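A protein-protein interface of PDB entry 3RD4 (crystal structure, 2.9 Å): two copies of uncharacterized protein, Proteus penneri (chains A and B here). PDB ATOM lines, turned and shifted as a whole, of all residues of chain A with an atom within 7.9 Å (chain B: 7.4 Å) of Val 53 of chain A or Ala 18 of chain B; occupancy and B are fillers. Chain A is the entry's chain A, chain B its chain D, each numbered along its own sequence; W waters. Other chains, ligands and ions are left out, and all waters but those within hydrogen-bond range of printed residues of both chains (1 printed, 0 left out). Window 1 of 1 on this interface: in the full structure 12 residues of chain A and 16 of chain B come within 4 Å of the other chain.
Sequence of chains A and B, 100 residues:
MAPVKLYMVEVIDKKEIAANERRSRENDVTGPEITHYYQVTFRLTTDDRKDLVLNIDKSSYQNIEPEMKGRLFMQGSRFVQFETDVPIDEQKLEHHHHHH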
ATOM      1  N   ASP A  13      16.508   7.972   0.214  1.00  0.00           N
ATOM      2  CA  ASP A  13      15.578   7.938  -0.908  1.00  0.00           C
ATOM      3  C   ASP A  13      14.113   8.022  -0.525  1.00  0.00           C
ATOM      4  O   ASP A  13      13.760   8.022   0.649  1.00  0.00           O
ATOM      5  CB  ASP A  13      15.780   6.658  -1.706  1.00  0.00           C
ATOM      6  CG  ASP A  13      15.989   6.922  -3.171  1.00  0.00           C
ATOM      7  OD1 ASP A  13      15.232   7.746  -3.742  1.00  0.00           O
ATOM      8  OD2 ASP A  13      16.911   6.298  -3.749  1.00  0.00           O
ATOM      9  N   LYS A  15      10.366   7.154  -3.046  1.00  0.00           N
ATOM     10  CA  LYS A  15       9.739   7.110  -4.366  1.00  0.00           C
ATOM     11  C   LYS A  15       8.545   6.154  -4.444  1.00  0.00           C
ATOM     12  O   LYS A  15       8.492   5.153  -3.729  1.00  0.00           O
ATOM     13  CB  LYS A  15      10.777   6.727  -5.431  1.00  0.00           C
ATOM     14  CG  LYS A  15      11.259   5.280  -5.365  1.00  0.00           C
ATOM     15  CD  LYS A  15      12.539   5.092  -6.179  1.00  0.00           C
ATOM     16  CE  LYS A  15      13.663   5.992  -5.635  1.00  0.00           C
ATOM     17  NZ  LYS A  15      14.975   5.817  -6.325  1.00  0.00           N
ATOM     18  N   ILE A  17       6.325   3.391  -6.413  1.00  0.00           N
ATOM     19  CA  ILE A  17       6.499   2.368  -7.426  1.00  0.00           C
ATOM     20  C   ILE A  17       5.114   1.838  -7.731  1.00  0.00           C
ATOM     21  O   ILE A  17       4.427   1.378  -6.823  1.00  0.00           O
ATOM     22  CB  ILE A  17       7.339   1.221  -6.887  1.00  0.00           C
ATOM     23  CG1 ILE A  17       8.667   1.759  -6.363  1.00  0.00           C
ATOM     24  CG2 ILE A  17       7.558   0.196  -7.962  1.00  0.00           C
ATOM     25  CD1 ILE A  17       9.496   0.723  -5.604  1.00  0.00           C
ATOM     26  N   TYR A  38       4.998   2.461  -1.581  1.00  0.00           N
ATOM     27  CA  TYR A  38       5.598   3.665  -1.040  1.00  0.00           C
ATOM     28  C   TYR A  38       6.863   3.215  -0.375  1.00  0.00           C
ATOM     29  O   TYR A  38       6.863   2.792   0.772  1.00  0.00           O
ATOM     30  CB  TYR A  38       4.653   4.318  -0.044  1.00  0.00           C
ATOM     31  CG  TYR A  38       3.404   4.826  -0.710  1.00  0.00           C
ATOM     32  CD1 TYR A  38       3.445   5.946  -1.537  1.00  0.00           C
ATOM     33  CD2 TYR A  38       2.181   4.181  -0.517  1.00  0.00           C
ATOM     34  CE1 TYR A  38       2.304   6.415  -2.146  1.00  0.00           C
ATOM     35  CE2 TYR A  38       1.028   4.637  -1.122  1.00  0.00           C
ATOM     36  CZ  TYR A  38       1.096   5.758  -1.933  1.00  0.00           C
ATOM     37  OH  TYR A  38      -0.055   6.245  -2.505  1.00  0.00           O
ATOM     38  N   GLN A  39       7.949   3.300  -1.118  1.00  0.00           N
ATOM     39  CA  GLN A  39       9.239   2.850  -0.637  1.00  0.00           C
ATOM     40  C   GLN A  39      10.181   3.983  -0.314  1.00  0.00           C
ATOM     41  O   GLN A  39      10.202   5.002  -0.996  1.00  0.00           O
ATOM     42  CB  GLN A  39       9.852   1.949  -1.699  1.00  0.00           C
ATOM     43  CG  GLN A  39      11.345   1.874  -1.692  1.00  0.00           C
ATOM     44  CD  GLN A  39      11.872   1.381  -3.017  1.00  0.00           C
ATOM     45  OE1 GLN A  39      12.466   2.137  -3.782  1.00  0.00           O
ATOM     46  NE2 GLN A  39      11.638   0.110  -3.306  1.00  0.00           N
ATOM     47  N   VAL A  40      10.959   3.807   0.742  1.00  0.00           N
ATOM     48  CA  VAL A  40      11.926   4.823   1.139  1.00  0.00           C
ATOM     49  C   VAL A  40      13.194   4.101   1.539  1.00  0.00           C
ATOM     50  O   VAL A  40      13.131   3.043   2.164  1.00  0.00           O
ATOM     51  CB  VAL A  40      11.409   5.692   2.313  1.00  0.00           C
ATOM     52  CG1 VAL A  40      10.622   4.858   3.271  1.00  0.00           C
ATOM     53  CG2 VAL A  40      12.574   6.323   3.051  1.00  0.00           C
ATOM     54  N   THR A  41      14.342   4.657   1.163  1.00  0.00           N
ATOM     55  CA  THR A  41      15.616   4.023   1.488  1.00  0.00           C
ATOM     56  C   THR A  41      16.250   4.636   2.724  1.00  0.00           C
ATOM     57  O   THR A  41      16.725   5.757   2.672  1.00  0.00           O
ATOM     58  CB  THR A  41      16.594   4.145   0.313  1.00  0.00           C
ATOM     59  OG1 THR A  41      15.932   3.745  -0.897  1.00  0.00           O
ATOM     60  CG2 THR A  41      17.796   3.261   0.537  1.00  0.00           C
ATOM     61  N   PHE A  42      16.244   3.916   3.838  1.00  0.00           N
ATOM     62  CA  PHE A  42      16.843   4.423   5.069  1.00  0.00           C
ATOM     63  C   PHE A  42      18.248   3.854   5.196  1.00  0.00           C
ATOM     64  O   PHE A  42      18.396   2.644   5.324  1.00  0.00           O
ATOM     65  CB  PHE A  42      16.067   3.966   6.311  1.00  0.00           C
ATOM     66  CG  PHE A  42      14.626   4.394   6.353  1.00  0.00           C
ATOM     67  CD1 PHE A  42      13.640   3.627   5.735  1.00  0.00           C
ATOM     68  CD2 PHE A  42      14.248   5.541   7.048  1.00  0.00           C
ATOM     69  CE1 PHE A  42      12.303   3.990   5.813  1.00  0.00           C
ATOM     70  CE2 PHE A  42      12.910   5.907   7.125  1.00  0.00           C
ATOM     71  CZ  PHE A  42      11.939   5.128   6.506  1.00  0.00           C
ATOM     72  N   ARG A  43      19.281   4.693   5.193  1.00  0.00           N
ATOM     73  CA  ARG A  43      20.646   4.171   5.320  1.00  0.00           C
ATOM     74  C   ARG A  43      21.130   4.203   6.758  1.00  0.00           C
ATOM     75  O   ARG A  43      21.037   5.237   7.408  1.00  0.00           O
ATOM     76  CB  ARG A  43      21.608   4.973   4.455  1.00  0.00           C
ATOM     77  CG  ARG A  43      23.061   4.579   4.627  1.00  0.00           C
ATOM     78  CD  ARG A  43      23.909   5.325   3.628  1.00  0.00           C
ATOM     79  NE  ARG A  43      23.446   5.065   2.276  1.00  0.00           N
ATOM     80  CZ  ARG A  43      23.441   5.973   1.315  1.00  0.00           C
ATOM     81  NH1 ARG A  43      23.883   7.198   1.570  1.00  0.00           N
ATOM     82  NH2 ARG A  43      22.986   5.663   0.110  1.00  0.00           N
ATOM     83  N   ARG A  49      27.962  -0.610   7.302  1.00  0.00           N
ATOM     84  CA  ARG A  49      27.399  -0.103   6.056  1.00  0.00           C
ATOM     85  C   ARG A  49      26.145  -0.861   5.620  1.00  0.00           C
ATOM     86  O   ARG A  49      26.234  -1.959   5.081  1.00  0.00           O
ATOM     87  CB  ARG A  49      28.464  -0.169   4.971  1.00  0.00           C
ATOM     88  CG  ARG A  49      29.889   0.023   5.498  1.00  0.00           C
ATOM     89  CD  ARG A  49      30.848   0.204   4.331  1.00  0.00           C
ATOM     90  NE  ARG A  49      32.267  -0.010   4.636  1.00  0.00           N
ATOM     91  CZ  ARG A  49      32.781  -1.108   5.192  1.00  0.00           C
ATOM     92  NH1 ARG A  49      31.999  -2.126   5.538  1.00  0.00           N
ATOM     93  NH2 ARG A  49      34.095  -1.197   5.376  1.00  0.00           N
ATOM     94  N   LYS A  50      24.972  -0.265   5.827  1.00  0.00           N
ATOM     95  CA  LYS A  50      23.725  -0.938   5.478  1.00  0.00           C
ATOM     96  C   LYS A  50      22.543  -0.014   5.132  1.00  0.00           C
ATOM     97  O   LYS A  50      22.263   0.952   5.840  1.00  0.00           O
ATOM     98  CB  LYS A  50      23.332  -1.875   6.631  1.00  0.00           C
ATOM     99  CG  LYS A  50      22.079  -2.685   6.374  1.00  0.00           C
ATOM    100  CD  LYS A  50      21.911  -3.862   7.346  1.00  0.00           C
ATOM    101  CE  LYS A  50      21.309  -3.449   8.694  1.00  0.00           C
ATOM    102  NZ  LYS A  50      20.827  -4.616   9.507  1.00  0.00           N
ATOM    103  N   ASP A  51      21.853  -0.315   4.036  1.00  0.00           N
ATOM    104  CA  ASP A  51      20.687   0.462   3.617  1.00  0.00           C
ATOM    105  C   ASP A  51      19.425  -0.389   3.752  1.00  0.00           C
ATOM    106  O   ASP A  51      19.432  -1.583   3.457  1.00  0.00           O
ATOM    107  CB  ASP A  51      20.811   0.893   2.159  1.00  0.00           C
ATOM    108  CG  ASP A  51      21.950   1.855   1.926  1.00  0.00           C
ATOM    109  OD1 ASP A  51      22.938   1.786   2.695  1.00  0.00           O
ATOM    110  OD2 ASP A  51      21.862   2.661   0.965  1.00  0.00           O
ATOM    111  N   LEU A  52      18.341   0.228   4.192  1.00  0.00           N
ATOM    112  CA  LEU A  52      17.082  -0.480   4.333  1.00  0.00           C
ATOM    113  C   LEU A  52      16.052   0.057   3.360  1.00  0.00           C
ATOM    114  O   LEU A  52      15.443   1.094   3.606  1.00  0.00           O
ATOM    115  CB  LEU A  52      16.518  -0.335   5.747  1.00  0.00           C
ATOM    116  CG  LEU A  52      17.118  -1.203   6.843  1.00  0.00           C
ATOM    117  CD1 LEU A  52      17.259  -2.616   6.315  1.00  0.00           C
ATOM    118  CD2 LEU A  52      18.462  -0.653   7.259  1.00  0.00           C
ATOM    119  N   VAL A  53      15.857  -0.625   2.244  1.00  0.00           N
ATOM    120  CA  VAL A  53      14.845  -0.173   1.305  1.00  0.00           C
ATOM    121  C   VAL A  53      13.553  -0.843   1.789  1.00  0.00           C
ATOM    122  O   VAL A  53      13.334  -2.036   1.562  1.00  0.00           O
ATOM    123  CB  VAL A  53      15.176  -0.611  -0.120  1.00  0.00           C
ATOM    124  CG1 VAL A  53      14.162  -0.035  -1.081  1.00  0.00           C
ATOM    125  CG2 VAL A  53      16.575  -0.144  -0.483  1.00  0.00           C
ATOM    126  N   LEU A  54      12.721  -0.064   2.481  1.00  0.00           N
ATOM    127  CA  LEU A  54      11.474  -0.551   3.051  1.00  0.00           C
ATOM    128  C   LEU A  54      10.203  -0.082   2.364  1.00  0.00           C
ATOM    129  O   LEU A  54      10.157   0.999   1.766  1.00  0.00           O
ATOM    130  CB  LEU A  54      11.390  -0.161   4.525  1.00  0.00           C
ATOM    131  CG  LEU A  54      12.531  -0.632   5.423  1.00  0.00           C
ATOM    132  CD1 LEU A  54      12.291  -0.163   6.860  1.00  0.00           C
ATOM    133  CD2 LEU A  54      12.648  -2.152   5.349  1.00  0.00           C
ATOM    134  N   ASN A  55       9.180  -0.938   2.454  1.00  0.00           N
ATOM    135  CA  ASN A  55       7.836  -0.687   1.922  1.00  0.00           C
ATOM    136  C   ASN A  55       7.137  -0.088   3.134  1.00  0.00           C
ATOM    137  O   ASN A  55       7.011  -0.777   4.154  1.00  0.00           O
ATOM    138  CB  ASN A  55       7.092  -1.993   1.591  1.00  0.00           C
ATOM    139  CG  ASN A  55       7.567  -2.666   0.306  1.00  0.00           C
ATOM    140  OD1 ASN A  55       7.659  -2.033  -0.750  1.00  0.00           O
ATOM    141  ND2 ASN A  55       7.838  -3.972   0.388  1.00  0.00           N
ATOM    142  N   ILE A  56       6.694   1.166   3.046  1.00  0.00           N
ATOM    143  CA  ILE A  56       6.001   1.788   4.167  1.00  0.00           C
ATOM    144  C   ILE A  56       4.646   2.340   3.745  1.00  0.00           C
ATOM    145  O   ILE A  56       4.327   2.359   2.560  1.00  0.00           O
ATOM    146  CB  ILE A  56       6.842   2.908   4.793  1.00  0.00           C
ATOM    147  CG1 ILE A  56       6.891   4.130   3.873  1.00  0.00           C
ATOM    148  CG2 ILE A  56       8.240   2.394   5.056  1.00  0.00           C
ATOM    149  CD1 ILE A  56       7.456   5.367   4.544  1.00  0.00           C
ATOM    150  N   LEU A  72      14.537   4.611  13.422  1.00  0.00           N
ATOM    151  CA  LEU A  72      13.722   3.713  12.619  1.00  0.00           C
ATOM    152  C   LEU A  72      13.356   2.493  13.450  1.00  0.00           C
ATOM    153  O   LEU A  72      14.238   1.799  13.967  1.00  0.00           O
ATOM    154  CB  LEU A  72      14.493   3.256  11.373  1.00  0.00           C
ATOM    155  CG  LEU A  72      13.767   2.282  10.442  1.00  0.00           C
ATOM    156  CD1 LEU A  72      12.635   2.981   9.749  1.00  0.00           C
ATOM    157  CD2 LEU A  72      14.710   1.752   9.421  1.00  0.00           C
ATOM    158  N   MET A  74      11.742  -1.148  13.381  1.00  0.00           N
ATOM    159  CA  MET A  74      11.355  -2.272  12.538  1.00  0.00           C
ATOM    160  C   MET A  74      10.965  -3.500  13.362  1.00  0.00           C
ATOM    161  O   MET A  74      11.477  -3.715  14.460  1.00  0.00           O
ATOM    162  CB  MET A  74      12.502  -2.670  11.606  1.00  0.00           C
ATOM    163  CG  MET A  74      12.813  -1.690  10.496  1.00  0.00           C
ATOM    164  SD  MET A  74      14.075  -2.394   9.398  1.00  0.00           S
ATOM    165  CE  MET A  74      13.076  -3.379   8.382  1.00  0.00           C
ATOM    166  N   GLY A  76      11.497  -6.808  12.693  1.00  0.00           N
ATOM    167  CA  GLY A  76      12.159  -7.737  11.810  1.00  0.00           C
ATOM    168  C   GLY A  76      12.439  -7.017  10.503  1.00  0.00           C
ATOM    169  O   GLY A  76      13.332  -6.173  10.421  1.00  0.00           O
ATOM    170  N   SER A  77      11.641  -7.316   9.490  1.00  0.00           N
ATOM    171  CA  SER A  77      11.821  -6.729   8.173  1.00  0.00           C
ATOM    172  C   SER A  77      10.685  -5.780   7.797  1.00  0.00           C
ATOM    173  O   SER A  77      10.623  -5.255   6.671  1.00  0.00           O
ATOM    174  CB  SER A  77      11.897  -7.869   7.187  1.00  0.00           C
ATOM    175  OG  SER A  77      10.909  -8.827   7.548  1.00  0.00           O
ATOM    176  N   GLU B  16      25.644  -3.325   2.331  1.00  0.00           N
ATOM    177  CA  GLU B  16      24.643  -4.359   2.524  1.00  0.00           C
ATOM    178  C   GLU B  16      23.301  -3.722   2.191  1.00  0.00           C
ATOM    179  O   GLU B  16      23.108  -2.532   2.419  1.00  0.00           O
ATOM    180  CB  GLU B  16      24.684  -4.783   3.983  1.00  0.00           C
ATOM    181  CG  GLU B  16      24.338  -6.213   4.244  1.00  0.00           C
ATOM    182  CD  GLU B  16      24.677  -6.621   5.666  1.00  0.00           C
ATOM    183  OE1 GLU B  16      25.872  -6.508   6.048  1.00  0.00           O
ATOM    184  OE2 GLU B  16      23.750  -7.049   6.391  1.00  0.00           O
ATOM    185  N   ILE B  17      22.362  -4.484   1.648  1.00  0.00           N
ATOM    186  CA  ILE B  17      21.074  -3.883   1.323  1.00  0.00           C
ATOM    187  C   ILE B  17      19.936  -4.807   1.668  1.00  0.00           C
ATOM    188  O   ILE B  17      19.737  -5.810   0.987  1.00  0.00           O
ATOM    189  CB  ILE B  17      20.978  -3.537  -0.178  1.00  0.00           C
ATOM    190  CG1 ILE B  17      22.083  -2.544  -0.555  1.00  0.00           C
ATOM    191  CG2 ILE B  17      19.609  -2.966  -0.487  1.00  0.00           C
ATOM    192  CD1 ILE B  17      22.395  -2.507  -2.029  1.00  0.00           C
ATOM    193  N   ALA B  18      19.206  -4.508   2.740  1.00  0.00           N
ATOM    194  CA  ALA B  18      18.059  -5.336   3.081  1.00  0.00           C
ATOM    195  C   ALA B  18      16.885  -4.612   2.430  1.00  0.00           C
ATOM    196  O   ALA B  18      16.560  -3.491   2.823  1.00  0.00           O
ATOM    197  CB  ALA B  18      17.875  -5.426   4.581  1.00  0.00           C
ATOM    198  N   ALA B  19      16.266  -5.227   1.415  1.00  0.00           N
ATOM    199  CA  ALA B  19      15.123  -4.598   0.722  1.00  0.00           C
ATOM    200  C   ALA B  19      13.811  -5.407   0.698  1.00  0.00           C
ATOM    201  O   ALA B  19      13.810  -6.554   0.262  1.00  0.00           O
ATOM    202  CB  ALA B  19      15.525  -4.247  -0.711  1.00  0.00           C
ATOM    203  N   ASN B  20      12.708  -4.802   1.164  1.00  0.00           N
ATOM    204  CA  ASN B  20      11.391  -5.462   1.160  1.00  0.00           C
ATOM    205  C   ASN B  20      11.040  -5.691  -0.313  1.00  0.00           C
ATOM    206  O   ASN B  20      11.373  -4.862  -1.169  1.00  0.00           O
ATOM    207  CB  ASN B  20      10.281  -4.574   1.764  1.00  0.00           C
ATOM    208  CG  ASN B  20      10.384  -4.402   3.268  1.00  0.00           C
ATOM    209  OD1 ASN B  20      10.989  -5.204   3.967  1.00  0.00           O
ATOM    210  ND2 ASN B  20       9.753  -3.354   3.775  1.00  0.00           N
ATOM    211  N   GLU B  21      10.365  -6.803  -0.609  1.00  0.00           N
ATOM    212  CA  GLU B  21       9.986  -7.129  -1.989  1.00  0.00           C
ATOM    213  C   GLU B  21       8.475  -6.962  -2.187  1.00  0.00           C
ATOM    214  O   GLU B  21       7.932  -5.886  -1.930  1.00  0.00           O
ATOM    215  CB  GLU B  21      10.405  -8.571  -2.328  1.00  0.00           C
ATOM    216  CG  GLU B  21      11.377  -8.708  -3.512  1.00  0.00           C
ATOM    217  CD  GLU B  21      12.833  -8.374  -3.161  1.00  0.00           C
ATOM    218  OE1 GLU B  21      13.100  -7.985  -2.006  1.00  0.00           O
ATOM    219  OE2 GLU B  21      13.718  -8.503  -4.040  1.00  0.00           O
ATOM    220  N   ILE B  34      11.625 -10.273   2.151  1.00  0.00           N
ATOM    221  CA  ILE B  34      12.761  -9.427   1.872  1.00  0.00           C
ATOM    222  C   ILE B  34      13.943 -10.192   1.294  1.00  0.00           C
ATOM    223  O   ILE B  34      14.064 -11.408   1.461  1.00  0.00           O
ATOM    224  CB  ILE B  34      13.201  -8.731   3.172  1.00  0.00           C
ATOM    225  CG1 ILE B  34      12.035  -7.931   3.745  1.00  0.00           C
ATOM    226  CG2 ILE B  34      14.407  -7.856   2.922  1.00  0.00           C
ATOM    227  CD1 ILE B  34      10.938  -8.791   4.310  1.00  0.00           C
ATOM    228  N   THR B  35      14.808  -9.457   0.603  1.00  0.00           N
ATOM    229  CA  THR B  35      16.011 -10.017   0.015  1.00  0.00           C
ATOM    230  C   THR B  35      17.193  -9.199   0.500  1.00  0.00           C
ATOM    231  O   THR B  35      17.246  -7.982   0.322  1.00  0.00           O
ATOM    232  CB  THR B  35      15.984  -9.956  -1.499  1.00  0.00           C
ATOM    233  OG1 THR B  35      14.752 -10.498  -1.970  1.00  0.00           O
ATOM    234  CG2 THR B  35      17.109 -10.775  -2.073  1.00  0.00           C
ATOM    235  N   HIS B  36      18.139  -9.891   1.115  1.00  0.00           N
ATOM    236  CA  HIS B  36      19.337  -9.279   1.652  1.00  0.00           C
ATOM    237  C   HIS B  36      20.406  -9.322   0.561  1.00  0.00           C
ATOM    238  O   HIS B  36      20.730 -10.394   0.055  1.00  0.00           O
ATOM    239  CB  HIS B  36      19.765 -10.092   2.866  1.00  0.00           C
ATOM    240  CG  HIS B  36      20.741  -9.404   3.766  1.00  0.00           C
ATOM    241  ND1 HIS B  36      20.609  -9.411   5.138  1.00  0.00           N
ATOM    242  CD2 HIS B  36      21.907  -8.766   3.503  1.00  0.00           C
ATOM    243  CE1 HIS B  36      21.654  -8.814   5.685  1.00  0.00           C
ATOM    244  NE2 HIS B  36      22.457  -8.414   4.715  1.00  0.00           N
ATOM    245  N   TYR B  37      20.935  -8.161   0.180  1.00  0.00           N
ATOM    246  CA  TYR B  37      21.968  -8.098  -0.852  1.00  0.00           C
ATOM    247  C   TYR B  37      23.313  -7.684  -0.272  1.00  0.00           C
ATOM    248  O   TYR B  37      23.381  -6.908   0.679  1.00  0.00           O
ATOM    249  CB  TYR B  37      21.577  -7.102  -1.943  1.00  0.00           C
ATOM    250  CG  TYR B  37      20.335  -7.490  -2.703  1.00  0.00           C
ATOM    251  CD1 TYR B  37      20.415  -8.209  -3.887  1.00  0.00           C
ATOM    252  CD2 TYR B  37      19.074  -7.179  -2.206  1.00  0.00           C
ATOM    253  CE1 TYR B  37      19.268  -8.607  -4.554  1.00  0.00           C
ATOM    254  CE2 TYR B  37      17.926  -7.575  -2.862  1.00  0.00           C
ATOM    255  CZ  TYR B  37      18.026  -8.293  -4.031  1.00  0.00           C
ATOM    256  OH  TYR B  37      16.872  -8.728  -4.657  1.00  0.00           O
ATOM    257  N   TYR B  38      24.385  -8.210  -0.844  1.00  0.00           N
ATOM    258  CA  TYR B  38      25.722  -7.862  -0.396  1.00  0.00           C
ATOM    259  C   TYR B  38      26.450  -7.415  -1.643  1.00  0.00           C
ATOM    260  O   TYR B  38      27.036  -8.241  -2.349  1.00  0.00           O
ATOM    261  CB  TYR B  38      26.425  -9.079   0.184  1.00  0.00           C
ATOM    262  CG  TYR B  38      25.714  -9.681   1.363  1.00  0.00           C
ATOM    263  CD1 TYR B  38      25.959  -9.226   2.648  1.00  0.00           C
ATOM    264  CD2 TYR B  38      24.798 -10.719   1.188  1.00  0.00           C
ATOM    265  CE1 TYR B  38      25.319  -9.793   3.732  1.00  0.00           C
ATOM    266  CE2 TYR B  38      24.149 -11.292   2.265  1.00  0.00           C
ATOM    267  CZ  TYR B  38      24.413 -10.827   3.537  1.00  0.00           C
ATOM    268  OH  TYR B  38      23.787 -11.392   4.630  1.00  0.00           O
HETATM  269  O   HOH W   1      23.200  -6.181   9.151  1.00  0.00           O
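Water W1 bridges NZ of Lys 50 of chain A (2.9 Å) and OE2 of Glu 16 of chain B (2.9 Å).
The backbone NH (N) of Val 40 of chain A lies within hydrogen-bond range of the backbone carbonyl oxygen (O) of Leu 54 of chain A (3.1 Å).
NE of Arg 43 of chain A is in salt-bridge range of OD2 of Asp 51 of chain A, 3.2 Å away.
The side-chain carboxylate (OE2) of Glu 16 of chain B lies within hydrogen-bond range of a ring nitrogen (NE2) of His 36 of chain B, 2.5 Å away.
O of Ala 19 of chain B lies within hydrogen-bond range of N of Thr 35 of chain B.
OE1 of Glu 21 of chain B is in hydrogen-bond range of OG1 of Thr 35 of chain B (3.0 Å).
The side-chain hydroxyl (OH) of Tyr 37 of chain B lies within hydrogen-bond range of the side-chain carboxylate (OE2) of Glu 21 of chain B, at 3.2 Å.
Of the printed residues of chain B, Val 53 of chain A touches Ala 18, Ala 19 and Asn 20.
Ala 18 of chain B touches just these residues of chain A: Asp 51 (3.0 Å), Leu 52 (3.4 Å) and Val 53 (3.0 Å).
Printed residues of chain A within 4 Å of Glu 21 of chain B: Asn 55 (3.0 Å).
Printed residues of chain A within 4 Å of Ile 34 of chain B: Ser 77 (3.2 Å).
Printed residues of chain B within 4 Å of Lys 50 of chain A: Glu 16 (3.5 Å).
The nearest printed residue of chain A that does not touch Glu 21 of chain B is Val 53 of chain A (6.0 Å).
Printed residues of chain B that touch a printed residue of chain A: Glu 16, Ile 17, Ala 18, Ala 19, Asn 20, Glu 21 and Ile 34.
Of the 21 printed residues of chain A, 8 touch a printed residue of chain B.
Among the printed residues, 14 pairs touch across the chains.
Lys 50 of chain A touches Glu 16 of chain B (CA to O, 3.5 Å).
Ile 17 of chain B touches Asp 51 of chain A.
CD1 of Leu 52 of chain A touches CB of Ala 18 of chain B, at 3.4 Å.
O of Val 53 of chain A touches CA of Ala 19 of chain B (3.2 Å).
CA of Leu 54 of chain A touches ND2 of Asn 20 of chain B (3.4 Å).
Ile 34 of chain B touches Ser 77 of chain A (CD1 to CB, 3.2 Å).
O of Arg 49 of chain A sits at hydrogen-bond distance from N of Glu 16 of chain B (3.1 Å).
The backbone NH of Asp 51 of chain A lies within hydrogen-bond range of the backbone carbonyl oxygen of Glu 16 of chain B, 3.0 Å away.
The backbone NH (N) of Ala 18 of chain B is in hydrogen-bond range of the backbone carbonyl oxygen (O) of Asp 51 of chain A (3.0 Å).
The backbone NH (N) of Val 53 of chain A sits at hydrogen-bond distance from the backbone carbonyl oxygen (O) of Ala 18 of chain B.
O of Val 53 of chain A is in hydrogen-bond range of N of Asn 20 of chain B (2.9 Å).
The side-chain amide nitrogen (ND2) of Asn 20 of chain B lies close to the backbone NH (N) of Asn 55 of chain A (2.8 Å).
ND2 of Asn 55 of chain A is in hydrogen-bond range of O of Glu 21 of chain B (3.0 Å).
The backbone carbonyl oxygen of Ser 77 of chain A lies close to the side-chain amide oxygen of Asn 20 of chain B, at 2.7 Å.
Positions printed for both chains: 17 and 38.
Of the 14 pairs that touch across the chains among the printed residues, none has its exchanged pair printed and touching as well.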
